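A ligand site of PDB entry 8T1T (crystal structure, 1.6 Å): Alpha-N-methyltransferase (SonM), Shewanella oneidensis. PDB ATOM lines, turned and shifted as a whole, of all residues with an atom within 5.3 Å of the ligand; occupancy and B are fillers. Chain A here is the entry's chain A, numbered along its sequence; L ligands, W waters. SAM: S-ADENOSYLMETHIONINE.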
ATOM      1  N   LEU A  11     -12.128 -22.585  12.244  1.00  0.00           N
ATOM      2  CA  LEU A  11     -11.628 -23.654  11.383  1.00  0.00           C
ATOM      3  C   LEU A  11     -12.780 -24.425  10.740  1.00  0.00           C
ATOM      4  O   LEU A  11     -12.691 -24.846   9.588  1.00  0.00           O
ATOM      5  CB  LEU A  11     -10.739 -24.591  12.215  1.00  0.00           C
ATOM      6  CG  LEU A  11      -9.273 -24.188  12.345  1.00  0.00           C
ATOM      7  CD1 LEU A  11      -8.605 -24.128  10.979  1.00  0.00           C
ATOM      8  CD2 LEU A  11      -9.144 -22.858  13.059  1.00  0.00           C
ATOM      9  N   TYR A  71       2.318 -11.737   0.604  1.00  0.00           N
ATOM     10  CA  TYR A  71       1.693 -11.041   1.725  1.00  0.00           C
ATOM     11  C   TYR A  71       1.596  -9.552   1.434  1.00  0.00           C
ATOM     12  O   TYR A  71       0.570  -8.935   1.703  1.00  0.00           O
ATOM     13  CB  TYR A  71       2.485 -11.297   3.013  1.00  0.00           C
ATOM     14  CG  TYR A  71       2.436 -12.709   3.521  1.00  0.00           C
ATOM     15  CD1 TYR A  71       1.416 -13.577   3.147  1.00  0.00           C
ATOM     16  CD2 TYR A  71       3.424 -13.204   4.360  1.00  0.00           C
ATOM     17  CE1 TYR A  71       1.367 -14.882   3.617  1.00  0.00           C
ATOM     18  CE2 TYR A  71       3.390 -14.503   4.824  1.00  0.00           C
ATOM     19  CZ  TYR A  71       2.358 -15.345   4.458  1.00  0.00           C
ATOM     20  OH  TYR A  71       2.315 -16.644   4.918  1.00  0.00           O
ATOM     21  N   TYR A  93      -9.229 -17.398   8.037  1.00  0.00           N
ATOM     22  CA  TYR A  93      -9.604 -18.588   8.779  1.00  0.00           C
ATOM     23  C   TYR A  93      -8.901 -18.562  10.136  1.00  0.00           C
ATOM     24  O   TYR A  93      -7.812 -17.989  10.275  1.00  0.00           O
ATOM     25  CB  TYR A  93      -9.324 -19.855   7.966  1.00  0.00           C
ATOM     26  CG  TYR A  93      -7.871 -20.264   7.868  1.00  0.00           C
ATOM     27  CD1 TYR A  93      -7.295 -21.058   8.841  1.00  0.00           C
ATOM     28  CD2 TYR A  93      -7.085 -19.856   6.804  1.00  0.00           C
ATOM     29  CE1 TYR A  93      -5.970 -21.443   8.755  1.00  0.00           C
ATOM     30  CE2 TYR A  93      -5.751 -20.225   6.706  1.00  0.00           C
ATOM     31  CZ  TYR A  93      -5.192 -21.033   7.687  1.00  0.00           C
ATOM     32  OH  TYR A  93      -3.871 -21.414   7.611  1.00  0.00           O
ATOM     33  N   GLY A  94      -9.566 -19.154  11.135  1.00  0.00           N
ATOM     34  CA  GLY A  94      -9.044 -19.231  12.490  1.00  0.00           C
ATOM     35  C   GLY A  94      -9.200 -17.896  13.232  1.00  0.00           C
ATOM     36  O   GLY A  94     -10.263 -17.278  13.194  1.00  0.00           O
ATOM     37  N   HIS A  95      -8.112 -17.475  13.887  1.00  0.00           N
ATOM     38  CA  HIS A  95      -7.973 -16.186  14.527  1.00  0.00           C
ATOM     39  C   HIS A  95      -7.131 -15.301  13.611  1.00  0.00           C
ATOM     40  O   HIS A  95      -6.068 -15.726  13.164  1.00  0.00           O
ATOM     41  CB  HIS A  95      -7.297 -16.381  15.902  1.00  0.00           C
ATOM     42  CG  HIS A  95      -7.117 -15.152  16.733  1.00  0.00           C
ATOM     43  ND1 HIS A  95      -6.584 -13.976  16.277  1.00  0.00           N
ATOM     44  CD2 HIS A  95      -7.376 -14.957  18.048  1.00  0.00           C
ATOM     45  CE1 HIS A  95      -6.552 -13.095  17.265  1.00  0.00           C
ATOM     46  NE2 HIS A  95      -7.013 -13.675  18.355  1.00  0.00           N
ATOM     47  N   PRO A  96      -7.572 -14.072  13.241  1.00  0.00           N
ATOM     48  CA  PRO A  96      -6.906 -13.329  12.166  1.00  0.00           C
ATOM     49  C   PRO A  96      -5.565 -12.741  12.590  1.00  0.00           C
ATOM     50  O   PRO A  96      -4.870 -12.145  11.777  1.00  0.00           O
ATOM     51  CB  PRO A  96      -7.919 -12.230  11.844  1.00  0.00           C
ATOM     52  CG  PRO A  96      -8.612 -11.967  13.166  1.00  0.00           C
ATOM     53  CD  PRO A  96      -8.687 -13.326  13.828  1.00  0.00           C
ATOM     54  N   VAL A  98      -3.304 -14.695  14.703  1.00  0.00           N
ATOM     55  CA  VAL A  98      -2.500 -15.791  15.216  1.00  0.00           C
ATOM     56  C   VAL A  98      -1.776 -16.478  14.058  1.00  0.00           C
ATOM     57  O   VAL A  98      -2.403 -17.094  13.198  1.00  0.00           O
ATOM     58  CB  VAL A  98      -3.361 -16.778  16.033  1.00  0.00           C
ATOM     59  CG1 VAL A  98      -2.624 -18.060  16.361  1.00  0.00           C
ATOM     60  CG2 VAL A  98      -3.893 -16.126  17.292  1.00  0.00           C
ATOM     61  N   PHE A  99      -0.434 -16.380  14.065  1.00  0.00           N
ATOM     62  CA  PHE A  99       0.391 -16.914  12.992  1.00  0.00           C
ATOM     63  C   PHE A  99      -0.149 -16.407  11.651  1.00  0.00           C
ATOM     64  O   PHE A  99      -0.313 -17.169  10.710  1.00  0.00           O
ATOM     65  CB  PHE A  99       0.481 -18.443  13.062  1.00  0.00           C
ATOM     66  CG  PHE A  99       1.372 -18.960  14.153  1.00  0.00           C
ATOM     67  CD1 PHE A  99       0.923 -19.092  15.448  1.00  0.00           C
ATOM     68  CD2 PHE A  99       2.705 -19.271  13.895  1.00  0.00           C
ATOM     69  CE1 PHE A  99       1.749 -19.559  16.457  1.00  0.00           C
ATOM     70  CE2 PHE A  99       3.531 -19.738  14.903  1.00  0.00           C
ATOM     71  CZ  PHE A  99       3.059 -19.870  16.176  1.00  0.00           C
ATOM     72  N   ALA A 100      -0.398 -15.088  11.593  1.00  0.00           N
ATOM     73  CA  ALA A 100      -0.999 -14.449  10.431  1.00  0.00           C
ATOM     74  C   ALA A 100      -0.527 -13.008  10.363  1.00  0.00           C
ATOM     75  O   ALA A 100      -0.937 -12.177  11.165  1.00  0.00           O
ATOM     76  CB  ALA A 100      -2.501 -14.533  10.542  1.00  0.00           C
ATOM     77  N   ILE A 123     -11.463 -18.154  16.729  1.00  0.00           N
ATOM     78  CA  ILE A 123     -11.045 -19.450  17.238  1.00  0.00           C
ATOM     79  C   ILE A 123      -9.922 -20.011  16.371  1.00  0.00           C
ATOM     80  O   ILE A 123     -10.113 -20.284  15.187  1.00  0.00           O
ATOM     81  CB  ILE A 123     -12.269 -20.389  17.292  1.00  0.00           C
ATOM     82  CG1 ILE A 123     -13.309 -19.870  18.295  1.00  0.00           C
ATOM     83  CG2 ILE A 123     -11.858 -21.820  17.580  1.00  0.00           C
ATOM     84  CD1 ILE A 123     -14.633 -20.607  18.243  1.00  0.00           C
ATOM     85  N   SER A 124      -8.744 -20.183  16.986  1.00  0.00           N
ATOM     86  CA  SER A 124      -7.527 -20.579  16.289  1.00  0.00           C
ATOM     87  C   SER A 124      -7.379 -22.106  16.292  1.00  0.00           C
ATOM     88  O   SER A 124      -8.149 -22.809  16.935  1.00  0.00           O
ATOM     89  CB  SER A 124      -6.304 -19.957  16.912  1.00  0.00           C
ATOM     90  OG  SER A 124      -6.002 -20.552  18.163  1.00  0.00           O
ATOM     91  N   ALA A 125      -6.357 -22.584  15.579  1.00  0.00           N
ATOM     92  CA  ALA A 125      -6.054 -24.005  15.525  1.00  0.00           C
ATOM     93  C   ALA A 125      -5.709 -24.515  16.916  1.00  0.00           C
ATOM     94  O   ALA A 125      -6.059 -25.646  17.267  1.00  0.00           O
ATOM     95  CB  ALA A 125      -4.925 -24.254  14.550  1.00  0.00           C
ATOM     96  N   GLU A 126      -5.013 -23.682  17.696  1.00  0.00           N
ATOM     97  CA  GLU A 126      -4.629 -23.997  19.059  1.00  0.00           C
ATOM     98  C   GLU A 126      -5.890 -24.233  19.901  1.00  0.00           C
ATOM     99  O   GLU A 126      -5.978 -25.210  20.643  1.00  0.00           O
ATOM    100  CB  GLU A 126      -3.779 -22.852  19.616  1.00  0.00           C
ATOM    101  CG  GLU A 126      -3.220 -23.110  21.005  1.00  0.00           C
ATOM    102  CD  GLU A 126      -2.340 -21.977  21.500  1.00  0.00           C
ATOM    103  OE1 GLU A 126      -1.264 -21.764  20.904  1.00  0.00           O
ATOM    104  OE2 GLU A 126      -2.747 -21.290  22.457  1.00  0.00           O
ATOM    105  N   LEU A 165       4.653 -26.860  17.519  1.00  0.00           N
ATOM    106  CA  LEU A 165       5.392 -26.331  16.380  1.00  0.00           C
ATOM    107  C   LEU A 165       4.434 -26.145  15.201  1.00  0.00           C
ATOM    108  O   LEU A 165       3.925 -27.123  14.639  1.00  0.00           O
ATOM    109  CB  LEU A 165       6.542 -27.274  16.028  1.00  0.00           C
ATOM    110  CG  LEU A 165       7.650 -27.399  17.081  1.00  0.00           C
ATOM    111  CD1 LEU A 165       8.786 -28.263  16.556  1.00  0.00           C
ATOM    112  CD2 LEU A 165       8.165 -26.037  17.488  1.00  0.00           C
ATOM    113  N   TRP A 166       4.180 -24.885  14.849  1.00  0.00           N
ATOM    114  CA  TRP A 166       3.286 -24.546  13.762  1.00  0.00           C
ATOM    115  C   TRP A 166       4.038 -24.572  12.431  1.00  0.00           C
ATOM    116  O   TRP A 166       5.261 -24.400  12.403  1.00  0.00           O
ATOM    117  CB  TRP A 166       2.649 -23.179  13.993  1.00  0.00           C
ATOM    118  CG  TRP A 166       1.843 -23.021  15.242  1.00  0.00           C
ATOM    119  CD1 TRP A 166       2.246 -23.209  16.535  1.00  0.00           C
ATOM    120  CD2 TRP A 166       0.485 -22.543  15.326  1.00  0.00           C
ATOM    121  NE1 TRP A 166       1.241 -22.909  17.411  1.00  0.00           N
ATOM    122  CE2 TRP A 166       0.144 -22.494  16.700  1.00  0.00           C
ATOM    123  CE3 TRP A 166      -0.475 -22.165  14.380  1.00  0.00           C
ATOM    124  CZ2 TRP A 166      -1.117 -22.086  17.131  1.00  0.00           C
ATOM    125  CZ3 TRP A 166      -1.718 -21.760  14.820  1.00  0.00           C
ATOM    126  CH2 TRP A 166      -2.030 -21.722  16.177  1.00  0.00           C
ATOM    127  N   GLN A 167       3.294 -24.726  11.344  1.00  0.00           N
ATOM    128  CA  GLN A 167       3.868 -24.711   9.996  1.00  0.00           C
ATOM    129  C   GLN A 167       4.985 -25.753   9.907  1.00  0.00           C
ATOM    130  O   GLN A 167       6.045 -25.511   9.328  1.00  0.00           O
ATOM    131  CB  GLN A 167       4.331 -23.290   9.653  1.00  0.00           C
ATOM    132  CG  GLN A 167       3.203 -22.274   9.758  1.00  0.00           C
ATOM    133  CD  GLN A 167       3.502 -20.873   9.288  1.00  0.00           C
ATOM    134  OE1 GLN A 167       4.632 -20.521   8.934  1.00  0.00           O
ATOM    135  NE2 GLN A 167       2.472 -20.044   9.284  1.00  0.00           N
ATOM    136  N   ILE A 168       4.727 -26.944  10.461  1.00  0.00           N
ATOM    137  CA  ILE A 168       5.713 -28.004  10.514  1.00  0.00           C
ATOM    138  C   ILE A 168       6.012 -28.506   9.106  1.00  0.00           C
ATOM    139  O   ILE A 168       7.126 -28.976   8.837  1.00  0.00           O
ATOM    140  CB  ILE A 168       5.253 -29.147  11.455  1.00  0.00           C
ATOM    141  CG1 ILE A 168       6.323 -30.233  11.625  1.00  0.00           C
ATOM    142  CG2 ILE A 168       3.921 -29.719  11.018  1.00  0.00           C
ATOM    143  CD1 ILE A 168       7.570 -29.782  12.355  1.00  0.00           C
ATOM    144  N   TYR A 206      -1.409 -33.035  14.381  1.00  0.00           N
ATOM    145  CA  TYR A 206      -2.791 -32.630  14.583  1.00  0.00           C
ATOM    146  C   TYR A 206      -3.292 -31.787  13.408  1.00  0.00           C
ATOM    147  O   TYR A 206      -2.620 -30.852  12.973  1.00  0.00           O
ATOM    148  CB  TYR A 206      -2.931 -31.844  15.884  1.00  0.00           C
ATOM    149  CG  TYR A 206      -4.292 -31.224  16.078  1.00  0.00           C
ATOM    150  CD1 TYR A 206      -5.412 -32.011  16.300  1.00  0.00           C
ATOM    151  CD2 TYR A 206      -4.482 -29.855  15.984  1.00  0.00           C
ATOM    152  CE1 TYR A 206      -6.669 -31.459  16.450  1.00  0.00           C
ATOM    153  CE2 TYR A 206      -5.729 -29.282  16.143  1.00  0.00           C
ATOM    154  CZ  TYR A 206      -6.834 -30.082  16.376  1.00  0.00           C
ATOM    155  OH  TYR A 206      -8.085 -29.540  16.533  1.00  0.00           O
ATOM    156  N   GLU A 207      -4.480 -32.131  12.923  1.00  0.00           N
ATOM    157  CA  GLU A 207      -5.209 -31.305  11.972  1.00  0.00           C
ATOM    158  C   GLU A 207      -6.672 -31.193  12.413  1.00  0.00           C
ATOM    159  O   GLU A 207      -7.395 -32.194  12.419  1.00  0.00           O
ATOM    160  CB  GLU A 207      -5.104 -31.866  10.552  1.00  0.00           C
ATOM    161  CG  GLU A 207      -3.685 -31.972  10.043  1.00  0.00           C
ATOM    162  CD  GLU A 207      -3.531 -32.757   8.759  1.00  0.00           C
ATOM    163  OE1 GLU A 207      -4.554 -33.274   8.260  1.00  0.00           O
ATOM    164  OE2 GLU A 207      -2.389 -32.883   8.279  1.00  0.00           O
ATOM    165  N   ALA A 208      -7.080 -29.985  12.794  1.00  0.00           N
ATOM    166  CA  ALA A 208      -8.477 -29.692  13.087  1.00  0.00           C
ATOM    167  C   ALA A 208      -9.290 -29.894  11.811  1.00  0.00           C
ATOM    168  O   ALA A 208      -8.831 -29.544  10.732  1.00  0.00           O
ATOM    169  CB  ALA A 208      -8.621 -28.287  13.601  1.00  0.00           C
ATOM    170  N   ALA A 209     -10.499 -30.433  11.962  1.00  0.00           N
ATOM    171  CA  ALA A 209     -11.406 -30.596  10.838  1.00  0.00           C
ATOM    172  C   ALA A 209     -11.903 -29.228  10.370  1.00  0.00           C
ATOM    173  O   ALA A 209     -12.177 -28.344  11.182  1.00  0.00           O
ATOM    174  CB  ALA A 209     -12.565 -31.495  11.219  1.00  0.00           C
ATOM    175  N   ASN A 210     -12.070 -29.096   9.044  1.00  0.00           N
ATOM    176  CA  ASN A 210     -12.640 -27.897   8.452  1.00  0.00           C
ATOM    177  C   ASN A 210     -14.095 -28.127   8.034  1.00  0.00           C
ATOM    178  O   ASN A 210     -14.807 -27.169   7.750  1.00  0.00           O
ATOM    179  CB  ASN A 210     -11.808 -27.427   7.249  1.00  0.00           C
ATOM    180  CG  ASN A 210     -10.403 -26.995   7.619  1.00  0.00           C
ATOM    181  OD1 ASN A 210     -10.214 -26.015   8.344  1.00  0.00           O
ATOM    182  ND2 ASN A 210      -9.402 -27.710   7.130  1.00  0.00           N
ATOM    183  N   PRO A 233       0.054 -28.536   4.642  1.00  0.00           N
ATOM    184  CA  PRO A 233       0.097 -27.144   5.074  1.00  0.00           C
ATOM    185  C   PRO A 233      -0.634 -26.863   6.384  1.00  0.00           C
ATOM    186  O   PRO A 233      -0.228 -25.976   7.127  1.00  0.00           O
ATOM    187  CB  PRO A 233      -0.587 -26.425   3.893  1.00  0.00           C
ATOM    188  CG  PRO A 233      -0.207 -27.260   2.685  1.00  0.00           C
ATOM    189  CD  PRO A 233      -0.228 -28.688   3.201  1.00  0.00           C
ATOM    190  N   ILE A 234      -1.704 -27.615   6.674  1.00  0.00           N
ATOM    191  CA  ILE A 234      -2.528 -27.313   7.841  1.00  0.00           C
ATOM    192  C   ILE A 234      -2.059 -28.093   9.072  1.00  0.00           C
ATOM    193  O   ILE A 234      -2.626 -27.932  10.141  1.00  0.00           O
ATOM    194  CB  ILE A 234      -4.023 -27.598   7.552  1.00  0.00           C
ATOM    195  CG1 ILE A 234      -4.278 -29.064   7.209  1.00  0.00           C
ATOM    196  CG2 ILE A 234      -4.554 -26.648   6.487  1.00  0.00           C
ATOM    197  CD1 ILE A 234      -5.750 -29.412   7.125  1.00  0.00           C
ATOM    198  N   SER A 235      -1.024 -28.926   8.929  1.00  0.00           N
ATOM    199  CA  SER A 235      -0.538 -29.741  10.030  1.00  0.00           C
ATOM    200  C   SER A 235       0.132 -28.883  11.112  1.00  0.00           C
ATOM    201  O   SER A 235       0.890 -27.959  10.814  1.00  0.00           O
ATOM    202  CB  SER A 235       0.421 -30.796   9.537  1.00  0.00           C
ATOM    203  OG  SER A 235      -0.169 -31.604   8.531  1.00  0.00           O
ATOM    204  N   THR A 236      -0.182 -29.192  12.383  1.00  0.00           N
ATOM    205  CA  THR A 236       0.537 -28.670  13.526  1.00  0.00           C
ATOM    206  C   THR A 236       1.109 -29.844  14.318  1.00  0.00           C
ATOM    207  O   THR A 236       0.451 -30.855  14.485  1.00  0.00           O
ATOM    208  CB  THR A 236      -0.375 -27.827  14.427  1.00  0.00           C
ATOM    209  OG1 THR A 236      -0.791 -26.649  13.729  1.00  0.00           O
ATOM    210  CG2 THR A 236       0.305 -27.399  15.712  1.00  0.00           C
HETATM  211  N   SAM L   1      -4.668 -17.918  11.818  1.00  0.00           N
HETATM  212  CA  SAM L   1      -4.638 -19.401  11.798  1.00  0.00           C
HETATM  213  C   SAM L   1      -5.195 -19.907  13.141  1.00  0.00           C
HETATM  214  O   SAM L   1      -5.027 -21.107  13.432  1.00  0.00           O
HETATM  215  OXT SAM L   1      -5.796 -19.070  13.852  1.00  0.00           O
HETATM  216  CB  SAM L   1      -3.212 -19.929  11.567  1.00  0.00           C
HETATM  217  CG  SAM L   1      -2.677 -19.700  10.149  1.00  0.00           C
HETATM  218  SD  SAM L   1      -0.895 -20.017   9.939  1.00  0.00           S
HETATM  219  CE  SAM L   1      -0.540 -19.068   8.463  1.00  0.00           C
HETATM  220  C5' SAM L   1      -0.947 -21.705   9.271  1.00  0.00           C
HETATM  221  C4' SAM L   1      -0.602 -22.739  10.325  1.00  0.00           C
HETATM  222  O4' SAM L   1      -1.663 -22.790  11.311  1.00  0.00           O
HETATM  223  C3' SAM L   1      -0.467 -24.177   9.841  1.00  0.00           C
HETATM  224  O3' SAM L   1       0.812 -24.429   9.283  1.00  0.00           O
HETATM  225  C2' SAM L   1      -0.691 -24.922  11.156  1.00  0.00           C
HETATM  226  O2' SAM L   1       0.446 -24.894  11.995  1.00  0.00           O
HETATM  227  C1' SAM L   1      -1.861 -24.122  11.733  1.00  0.00           C
HETATM  228  N9  SAM L   1      -3.130 -24.607  11.237  1.00  0.00           N
HETATM  229  C8  SAM L   1      -3.886 -24.098  10.212  1.00  0.00           C
HETATM  230  N7  SAM L   1      -4.965 -24.808   9.951  1.00  0.00           N
HETATM  231  C5  SAM L   1      -4.895 -25.862  10.851  1.00  0.00           C
HETATM  232  C6  SAM L   1      -5.735 -26.971  11.084  1.00  0.00           C
HETATM  233  N6  SAM L   1      -6.867 -27.195  10.409  1.00  0.00           N
HETATM  234  N1  SAM L   1      -5.388 -27.832  12.067  1.00  0.00           N
HETATM  235  C2  SAM L   1      -4.254 -27.599  12.741  1.00  0.00           C
HETATM  236  N3  SAM L   1      -3.382 -26.598  12.618  1.00  0.00           N
HETATM  237  C4  SAM L   1      -3.771 -25.757  11.645  1.00  0.00           C
HETATM  238  O   HOH W   1      -7.384 -25.006   8.326  1.00  0.00           O
HETATM  239  O   HOH W   2      -5.332 -17.182   9.160  1.00  0.00           O
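The backbone carbonyl oxygen (O) of Phe 99 sits close to a sulfur (SD) of the ligand (3.0 Å).
N3 of the ligand sits close to O of Ile 234, at 2.9 Å.
Merely in contact with the ligand: Leu 11 (3.6 Å), Tyr 93 (3.3 Å), Gly 94 (3.5 Å), Ser 124 (3.2 Å), Trp 166 (3.3 Å), Tyr 206 (3.6 Å) and Glu 207 (3.5 Å).
Hydrophobic or aromatic side chains that line the ligand: Leu 11, Tyr 93, His 95, Val 98, Phe 99, Ala 125, Trp 166, Tyr 206, Ala 208 and Ile 234.
Within 4 Å of the ligand: Leu 11, Tyr 93, Gly 94, His 95, Val 98, Phe 99, Ser 124, Ala 125, Trp 166, Gln 167, Tyr 206, Glu 207, Ala 208, Pro 233, Ile 234, Ser 235 and Thr 236.
Water W2 lies within hydrogen-bond range of O of Tyr 93 and N of the ligand.
Water W1 bridges N7 of the ligand (2.9 Å) and OD1 of Asn 210 (3.0 Å).
The side-chain amide oxygen (OD1) of Asn 210 lies close to the backbone carbonyl oxygen (O) of Leu 11 (3.0 Å).
The side-chain hydroxyl of Ser 235 is in hydrogen-bond range of the side-chain carboxylate of Glu 207 (2.6 Å).
The backbone NH (N) of Glu 126 lies close to the side-chain hydroxyl (OG) of Ser 124, at 3.3 Å.
O of Thr 236 is in hydrogen-bond range of N of Tyr 206 (2.9 Å).
N of the ligand sits at hydrogen-bond distance from O of His 95 (2.9 Å).
N of Ala 125 is in hydrogen-bond range of O of the ligand (2.9 Å).
The backbone carbonyl oxygen of Ala 208 sits at hydrogen-bond distance from a nitrogen (N6) of the ligand (3.1 Å).
The backbone carbonyl oxygen of Ser 235 is in hydrogen-bond range of an oxygen (O2') of the ligand, 3.3 Å away.
O2' of the ligand is in hydrogen-bond range of OG1 of Thr 236 (2.8 Å).
O of Pro 233 lies within hydrogen-bond range of O3' of the ligand (2.9 Å).
The backbone NH (N) of Gln 167 sits at hydrogen-bond distance from an oxygen (O2') of the ligand, at 2.9 Å.
N of the ligand sits at hydrogen-bond distance from O of Val 98 (2.8 Å).
N1 of the ligand is in hydrogen-bond range of N of Ala 208 (2.8 Å).
The backbone NH (N) of His 95 lies within hydrogen-bond range of an oxygen (OXT) of the ligand (2.8 Å).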
